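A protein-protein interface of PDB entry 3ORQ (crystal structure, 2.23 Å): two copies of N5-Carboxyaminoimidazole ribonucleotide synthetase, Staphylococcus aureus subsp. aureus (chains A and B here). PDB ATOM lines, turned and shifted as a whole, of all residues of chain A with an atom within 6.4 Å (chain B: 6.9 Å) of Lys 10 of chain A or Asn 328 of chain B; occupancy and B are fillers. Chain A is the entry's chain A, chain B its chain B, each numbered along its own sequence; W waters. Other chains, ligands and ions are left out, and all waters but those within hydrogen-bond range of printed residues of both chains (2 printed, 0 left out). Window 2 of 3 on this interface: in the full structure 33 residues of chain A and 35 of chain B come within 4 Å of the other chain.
The backbone carbonyl oxygen of Thr 299 of chain A lies within hydrogen-bond range of the side-chain amide nitrogen of Gln 301 of chain A (3.1 Å). The side-chain amide oxygen of Asn 331 of chain B sits close to the backbone carbonyl oxygen of Asn 328 of chain B, at 3.1 Å. The backbone carbonyl oxygen (O) of Leu 9 of chain A lies within hydrogen-bond range of the side-chain amide nitrogen (NE2) of Gln 301 of chain A (2.7 Å).
Lys 10 of chain A touches Asn 328 of chain B. Phe 11 of chain A touches Glu 327 of chain B (CZ to OE1, 3.5 Å). OE1 of Gln 301 of chain A touches CA of Asn 331 of chain B (3.1 Å).
Leu 9 of chain A touches none of the printed residues of chain B. Of chain B, only Asn 328 (3.2 Å) comes within 4 Å of Lys 10 of chain A. Of the printed residues of chain B, Phe 11 of chain A touches Glu 327 (3.5 Å). Of the printed residues of chain B, Gln 301 of chain A touches Asn 331. Leu 323 of chain B touches none of the printed residues of chain A. Printed residues of chain A within 4 Å of Glu 327 of chain B: Phe 11. Asn 328 of chain B touches just one residue of chain A: Lys 10. Of the printed residues of chain A, Asn 331 of chain B touches Gln 301 (3.1 Å). The nearest printed residue of chain A that does not touch Asn 328 of chain B is Phe 11 of chain A (6.9 Å).
Printed residues of chain A that touch a printed residue of chain B: Lys 10, Phe 11 and Gln 301. Of the 10 printed residues of chain B, 3 touch a printed residue of chain A. Among the printed residues, no Asp or Glu carboxylate lies within 4 Å of a Lys or Arg side-chain nitrogen of the other chain.
No position is printed for both chains. Of the 3 pairs that touch across the chains among the printed residues, none has its exchanged pair printed and touching as well.
Water W1 bridges OE1 of Gln 301 of chain A (2.8 Å) and O of Phe 330 of chain B (3.4 Å). Water W2 lies within hydrogen-bond range of the backbone carbonyl oxygen (O) of Asn 328 of chain B (2.8 Å) and the side-chain amino group (NZ) of Lys 10 of chain A (3.0 Å).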
ATOM      1  N   LYS A   8      34.855   2.468  -7.528  1.00  0.00           N
ATOM      2  CA  LYS A   8      34.091   1.544  -6.702  1.00  0.00           C
ATOM      3  C   LYS A   8      32.765   1.293  -7.391  1.00  0.00           C
ATOM      4  O   LYS A   8      31.922   2.188  -7.454  1.00  0.00           O
ATOM      5  CB  LYS A   8      33.898   2.071  -5.261  1.00  0.00           C
ATOM      6  CG  LYS A   8      35.225   2.087  -4.462  1.00  0.00           C
ATOM      7  CD  LYS A   8      35.078   2.652  -3.035  1.00  0.00           C
ATOM      8  CE  LYS A   8      36.462   2.653  -2.330  1.00  0.00           C
ATOM      9  NZ  LYS A   8      36.619   3.538  -1.129  1.00  0.00           N
ATOM     10  N   LEU A   9      32.601   0.090  -7.948  1.00  0.00           N
ATOM     11  CA  LEU A   9      31.373  -0.261  -8.694  1.00  0.00           C
ATOM     12  C   LEU A   9      30.392  -1.034  -7.823  1.00  0.00           C
ATOM     13  O   LEU A   9      30.778  -1.996  -7.121  1.00  0.00           O
ATOM     14  CB  LEU A   9      31.691  -1.108  -9.934  1.00  0.00           C
ATOM     15  CG  LEU A   9      32.631  -0.475 -10.967  1.00  0.00           C
ATOM     16  CD1 LEU A   9      32.987  -1.534 -11.977  1.00  0.00           C
ATOM     17  CD2 LEU A   9      32.004   0.784 -11.595  1.00  0.00           C
ATOM     18  N   LYS A  10      29.126  -0.646  -7.902  1.00  0.00           N
ATOM     19  CA  LYS A  10      28.067  -1.263  -7.104  1.00  0.00           C
ATOM     20  C   LYS A  10      27.314  -2.278  -7.921  1.00  0.00           C
ATOM     21  O   LYS A  10      27.323  -2.239  -9.174  1.00  0.00           O
ATOM     22  CB  LYS A  10      27.106  -0.191  -6.552  1.00  0.00           C
ATOM     23  CG  LYS A  10      27.800   0.775  -5.500  1.00  0.00           C
ATOM     24  CD  LYS A  10      26.869   1.934  -5.152  1.00  0.00           C
ATOM     25  CE  LYS A  10      27.189   2.530  -3.797  1.00  0.00           C
ATOM     26  NZ  LYS A  10      28.350   3.442  -3.859  1.00  0.00           N
ATOM     27  N   PHE A  11      26.667  -3.216  -7.229  1.00  0.00           N
ATOM     28  CA  PHE A  11      25.938  -4.242  -7.929  1.00  0.00           C
ATOM     29  C   PHE A  11      25.079  -3.565  -8.983  1.00  0.00           C
ATOM     30  O   PHE A  11      24.639  -2.412  -8.789  1.00  0.00           O
ATOM     31  CB  PHE A  11      25.092  -5.106  -6.973  1.00  0.00           C
ATOM     32  CG  PHE A  11      23.994  -4.340  -6.260  1.00  0.00           C
ATOM     33  CD1 PHE A  11      22.818  -3.992  -6.925  1.00  0.00           C
ATOM     34  CD2 PHE A  11      24.146  -3.967  -4.928  1.00  0.00           C
ATOM     35  CE1 PHE A  11      21.802  -3.311  -6.258  1.00  0.00           C
ATOM     36  CE2 PHE A  11      23.119  -3.299  -4.244  1.00  0.00           C
ATOM     37  CZ  PHE A  11      21.970  -2.968  -4.892  1.00  0.00           C
ATOM     38  N   GLY A  12      24.819  -4.272 -10.088  1.00  0.00           N
ATOM     39  CA  GLY A  12      24.076  -3.658 -11.191  1.00  0.00           C
ATOM     40  C   GLY A  12      25.012  -3.165 -12.274  1.00  0.00           C
ATOM     41  O   GLY A  12      24.597  -3.007 -13.420  1.00  0.00           O
ATOM     42  N   ALA A  13      26.296  -2.952 -11.949  1.00  0.00           N
ATOM     43  CA  ALA A  13      27.237  -2.528 -12.976  1.00  0.00           C
ATOM     44  C   ALA A  13      27.597  -3.731 -13.847  1.00  0.00           C
ATOM     45  O   ALA A  13      27.290  -4.891 -13.487  1.00  0.00           O
ATOM     46  CB  ALA A  13      28.459  -1.951 -12.352  1.00  0.00           C
ATOM     47  N   THR A  14      28.236  -3.458 -14.988  1.00  0.00           N
ATOM     48  CA  THR A  14      28.589  -4.489 -15.933  1.00  0.00           C
ATOM     49  C   THR A  14      30.093  -4.787 -16.011  1.00  0.00           C
ATOM     50  O   THR A  14      30.915  -3.895 -16.181  1.00  0.00           O
ATOM     51  CB  THR A  14      28.098  -4.108 -17.332  1.00  0.00           C
ATOM     52  OG1 THR A  14      26.668  -3.913 -17.296  1.00  0.00           O
ATOM     53  CG2 THR A  14      28.435  -5.233 -18.305  1.00  0.00           C
ATOM     54  N   GLY A  35      25.446  -9.972  -8.210  1.00  0.00           N
ATOM     55  CA  GLY A  35      24.543  -8.986  -8.835  1.00  0.00           C
ATOM     56  C   GLY A  35      25.182  -8.043  -9.862  1.00  0.00           C
ATOM     57  O   GLY A  35      24.634  -6.979 -10.124  1.00  0.00           O
ATOM     58  N   TYR A  36      26.325  -8.439 -10.430  1.00  0.00           N
ATOM     59  CA  TYR A  36      26.920  -7.755 -11.585  1.00  0.00           C
ATOM     60  C   TYR A  36      26.465  -8.437 -12.888  1.00  0.00           C
ATOM     61  O   TYR A  36      26.230  -9.652 -12.925  1.00  0.00           O
ATOM     62  CB  TYR A  36      28.461  -7.784 -11.499  1.00  0.00           C
ATOM     63  CG  TYR A  36      28.953  -6.980 -10.326  1.00  0.00           C
ATOM     64  CD1 TYR A  36      29.051  -5.607 -10.415  1.00  0.00           C
ATOM     65  CD2 TYR A  36      29.261  -7.587  -9.115  1.00  0.00           C
ATOM     66  CE1 TYR A  36      29.455  -4.847  -9.344  1.00  0.00           C
ATOM     67  CE2 TYR A  36      29.673  -6.827  -8.016  1.00  0.00           C
ATOM     68  CZ  TYR A  36      29.736  -5.447  -8.143  1.00  0.00           C
ATOM     69  OH  TYR A  36      30.141  -4.655  -7.095  1.00  0.00           O
ATOM     70  N   THR A 299      36.110  -4.767  -8.997  1.00  0.00           N
ATOM     71  CA  THR A 299      35.000  -3.806  -8.874  1.00  0.00           C
ATOM     72  C   THR A 299      35.316  -2.783  -7.782  1.00  0.00           C
ATOM     73  O   THR A 299      34.484  -1.911  -7.469  1.00  0.00           O
ATOM     74  CB  THR A 299      33.635  -4.496  -8.564  1.00  0.00           C
ATOM     75  OG1 THR A 299      33.739  -5.262  -7.334  1.00  0.00           O
ATOM     76  CG2 THR A 299      33.212  -5.449  -9.739  1.00  0.00           C
ATOM     77  N   GLN A 301      35.974  -3.136  -4.472  1.00  0.00           N
ATOM     78  CA  GLN A 301      35.450  -3.347  -3.115  1.00  0.00           C
ATOM     79  C   GLN A 301      36.582  -3.655  -2.138  1.00  0.00           C
ATOM     80  O   GLN A 301      37.690  -3.964  -2.547  1.00  0.00           O
ATOM     81  CB  GLN A 301      34.461  -4.520  -3.084  1.00  0.00           C
ATOM     82  CG  GLN A 301      33.368  -4.538  -4.228  1.00  0.00           C
ATOM     83  CD  GLN A 301      32.476  -3.383  -4.151  1.00  0.00           C
ATOM     84  OE1 GLN A 301      31.716  -3.237  -3.195  1.00  0.00           O
ATOM     85  NE2 GLN A 301      32.560  -2.505  -5.140  1.00  0.00           N
ATOM     86  N   LEU B 323      18.131  -2.737   1.242  1.00  0.00           N
ATOM     87  CA  LEU B 323      19.039  -2.127   0.288  1.00  0.00           C
ATOM     88  C   LEU B 323      19.047  -0.606   0.471  1.00  0.00           C
ATOM     89  O   LEU B 323      20.105   0.006   0.570  1.00  0.00           O
ATOM     90  CB  LEU B 323      18.678  -2.500  -1.163  1.00  0.00           C
ATOM     91  CG  LEU B 323      18.764  -3.983  -1.554  1.00  0.00           C
ATOM     92  CD1 LEU B 323      18.492  -4.201  -3.083  1.00  0.00           C
ATOM     93  CD2 LEU B 323      20.098  -4.601  -1.159  1.00  0.00           C
ATOM     94  N   ASP B 324      17.877   0.002   0.536  1.00  0.00           N
ATOM     95  CA  ASP B 324      17.786   1.440   0.752  1.00  0.00           C
ATOM     96  C   ASP B 324      18.635   1.851   1.964  1.00  0.00           C
ATOM     97  O   ASP B 324      19.300   2.897   1.974  1.00  0.00           O
ATOM     98  CB  ASP B 324      16.333   1.893   0.978  1.00  0.00           C
ATOM     99  CG  ASP B 324      15.465   1.780  -0.263  1.00  0.00           C
ATOM    100  OD1 ASP B 324      16.028   1.809  -1.387  1.00  0.00           O
ATOM    101  OD2 ASP B 324      14.205   1.676  -0.109  1.00  0.00           O
ATOM    102  N   LEU B 325      18.626   1.018   2.983  1.00  0.00           N
ATOM    103  CA  LEU B 325      19.332   1.381   4.197  1.00  0.00           C
ATOM    104  C   LEU B 325      20.832   1.142   4.092  1.00  0.00           C
ATOM    105  O   LEU B 325      21.606   1.985   4.525  1.00  0.00           O
ATOM    106  CB  LEU B 325      18.810   0.587   5.383  1.00  0.00           C
ATOM    107  CG  LEU B 325      19.559   0.829   6.694  1.00  0.00           C
ATOM    108  CD1 LEU B 325      19.348   2.325   7.201  1.00  0.00           C
ATOM    109  CD2 LEU B 325      19.142  -0.173   7.779  1.00  0.00           C
ATOM    110  N   LEU B 326      21.226  -0.014   3.535  1.00  0.00           N
ATOM    111  CA  LEU B 326      22.552  -0.542   3.721  1.00  0.00           C
ATOM    112  C   LEU B 326      23.446  -0.571   2.460  1.00  0.00           C
ATOM    113  O   LEU B 326      24.658  -0.823   2.577  1.00  0.00           O
ATOM    114  CB  LEU B 326      22.433  -1.974   4.265  1.00  0.00           C
ATOM    115  CG  LEU B 326      21.888  -2.186   5.691  1.00  0.00           C
ATOM    116  CD1 LEU B 326      21.741  -3.647   6.032  1.00  0.00           C
ATOM    117  CD2 LEU B 326      22.693  -1.423   6.800  1.00  0.00           C
ATOM    118  N   GLU B 327      22.882  -0.377   1.268  1.00  0.00           N
ATOM    119  CA  GLU B 327      23.670  -0.675   0.063  1.00  0.00           C
ATOM    120  C   GLU B 327      24.974   0.132  -0.013  1.00  0.00           C
ATOM    121  O   GLU B 327      26.002  -0.337  -0.559  1.00  0.00           O
ATOM    122  CB  GLU B 327      22.835  -0.491  -1.226  1.00  0.00           C
ATOM    123  CG  GLU B 327      22.287   0.921  -1.394  1.00  0.00           C
ATOM    124  CD  GLU B 327      21.338   1.055  -2.601  1.00  0.00           C
ATOM    125  OE1 GLU B 327      21.431   0.231  -3.548  1.00  0.00           O
ATOM    126  OE2 GLU B 327      20.533   1.996  -2.606  1.00  0.00           O
ATOM    127  N   ASN B 328      24.953   1.346   0.515  1.00  0.00           N
ATOM    128  CA  ASN B 328      26.175   2.178   0.492  1.00  0.00           C
ATOM    129  C   ASN B 328      27.329   1.708   1.380  1.00  0.00           C
ATOM    130  O   ASN B 328      28.449   2.123   1.174  1.00  0.00           O
ATOM    131  CB  ASN B 328      25.855   3.670   0.743  1.00  0.00           C
ATOM    132  CG  ASN B 328      25.092   4.272  -0.424  1.00  0.00           C
ATOM    133  OD1 ASN B 328      25.225   3.805  -1.575  1.00  0.00           O
ATOM    134  ND2 ASN B 328      24.284   5.280  -0.147  1.00  0.00           N
ATOM    135  N   GLU B 329      27.080   0.799   2.315  1.00  0.00           N
ATOM    136  CA  GLU B 329      28.189   0.201   3.033  1.00  0.00           C
ATOM    137  C   GLU B 329      28.615  -1.210   2.627  1.00  0.00           C
ATOM    138  O   GLU B 329      29.501  -1.754   3.264  1.00  0.00           O
ATOM    139  CB  GLU B 329      27.983   0.295   4.547  1.00  0.00           C
ATOM    140  CG  GLU B 329      26.698  -0.268   5.070  1.00  0.00           C
ATOM    141  CD  GLU B 329      26.439   0.212   6.485  1.00  0.00           C
ATOM    142  OE1 GLU B 329      27.174  -0.209   7.394  1.00  0.00           O
ATOM    143  OE2 GLU B 329      25.527   1.032   6.689  1.00  0.00           O
ATOM    144  N   PHE B 330      28.042  -1.780   1.555  1.00  0.00           N
ATOM    145  CA  PHE B 330      28.396  -3.164   1.143  1.00  0.00           C
ATOM    146  C   PHE B 330      29.859  -3.294   0.793  1.00  0.00           C
ATOM    147  O   PHE B 330      30.505  -4.282   1.125  1.00  0.00           O
ATOM    148  CB  PHE B 330      27.543  -3.646  -0.043  1.00  0.00           C
ATOM    149  CG  PHE B 330      26.097  -3.954   0.331  1.00  0.00           C
ATOM    150  CD1 PHE B 330      25.736  -4.133   1.667  1.00  0.00           C
ATOM    151  CD2 PHE B 330      25.122  -4.037  -0.633  1.00  0.00           C
ATOM    152  CE1 PHE B 330      24.395  -4.436   2.037  1.00  0.00           C
ATOM    153  CE2 PHE B 330      23.799  -4.364  -0.280  1.00  0.00           C
ATOM    154  CZ  PHE B 330      23.447  -4.532   1.063  1.00  0.00           C
ATOM    155  N   ASN B 331      30.381  -2.261   0.155  1.00  0.00           N
ATOM    156  CA  ASN B 331      31.774  -2.227  -0.282  1.00  0.00           C
ATOM    157  C   ASN B 331      32.791  -2.430   0.869  1.00  0.00           C
ATOM    158  O   ASN B 331      33.893  -2.896   0.643  1.00  0.00           O
ATOM    159  CB  ASN B 331      32.075  -0.916  -1.024  1.00  0.00           C
ATOM    160  CG  ASN B 331      32.086   0.294  -0.091  1.00  0.00           C
ATOM    161  OD1 ASN B 331      31.054   0.872   0.185  1.00  0.00           O
ATOM    162  ND2 ASN B 331      33.266   0.659   0.404  1.00  0.00           N
ATOM    163  N   GLU B 332      32.387  -2.099   2.087  1.00  0.00           N
ATOM    164  CA  GLU B 332      33.290  -2.115   3.224  1.00  0.00           C
ATOM    165  C   GLU B 332      33.243  -3.461   3.934  1.00  0.00           C
ATOM    166  O   GLU B 332      34.034  -3.716   4.855  1.00  0.00           O
ATOM    167  CB  GLU B 332      32.882  -1.004   4.203  1.00  0.00           C
ATOM    168  CG  GLU B 332      33.365   0.396   3.794  1.00  0.00           C
ATOM    169  CD  GLU B 332      32.417   1.495   4.287  1.00  0.00           C
ATOM    170  OE1 GLU B 332      31.823   1.308   5.375  1.00  0.00           O
ATOM    171  OE2 GLU B 332      32.205   2.511   3.547  1.00  0.00           O
HETATM  172  O   HOH W   1      30.314  -5.393  -2.094  1.00  0.00           O
HETATM  173  O   HOH W   2      29.225   3.737  -1.029  1.00  0.00           O
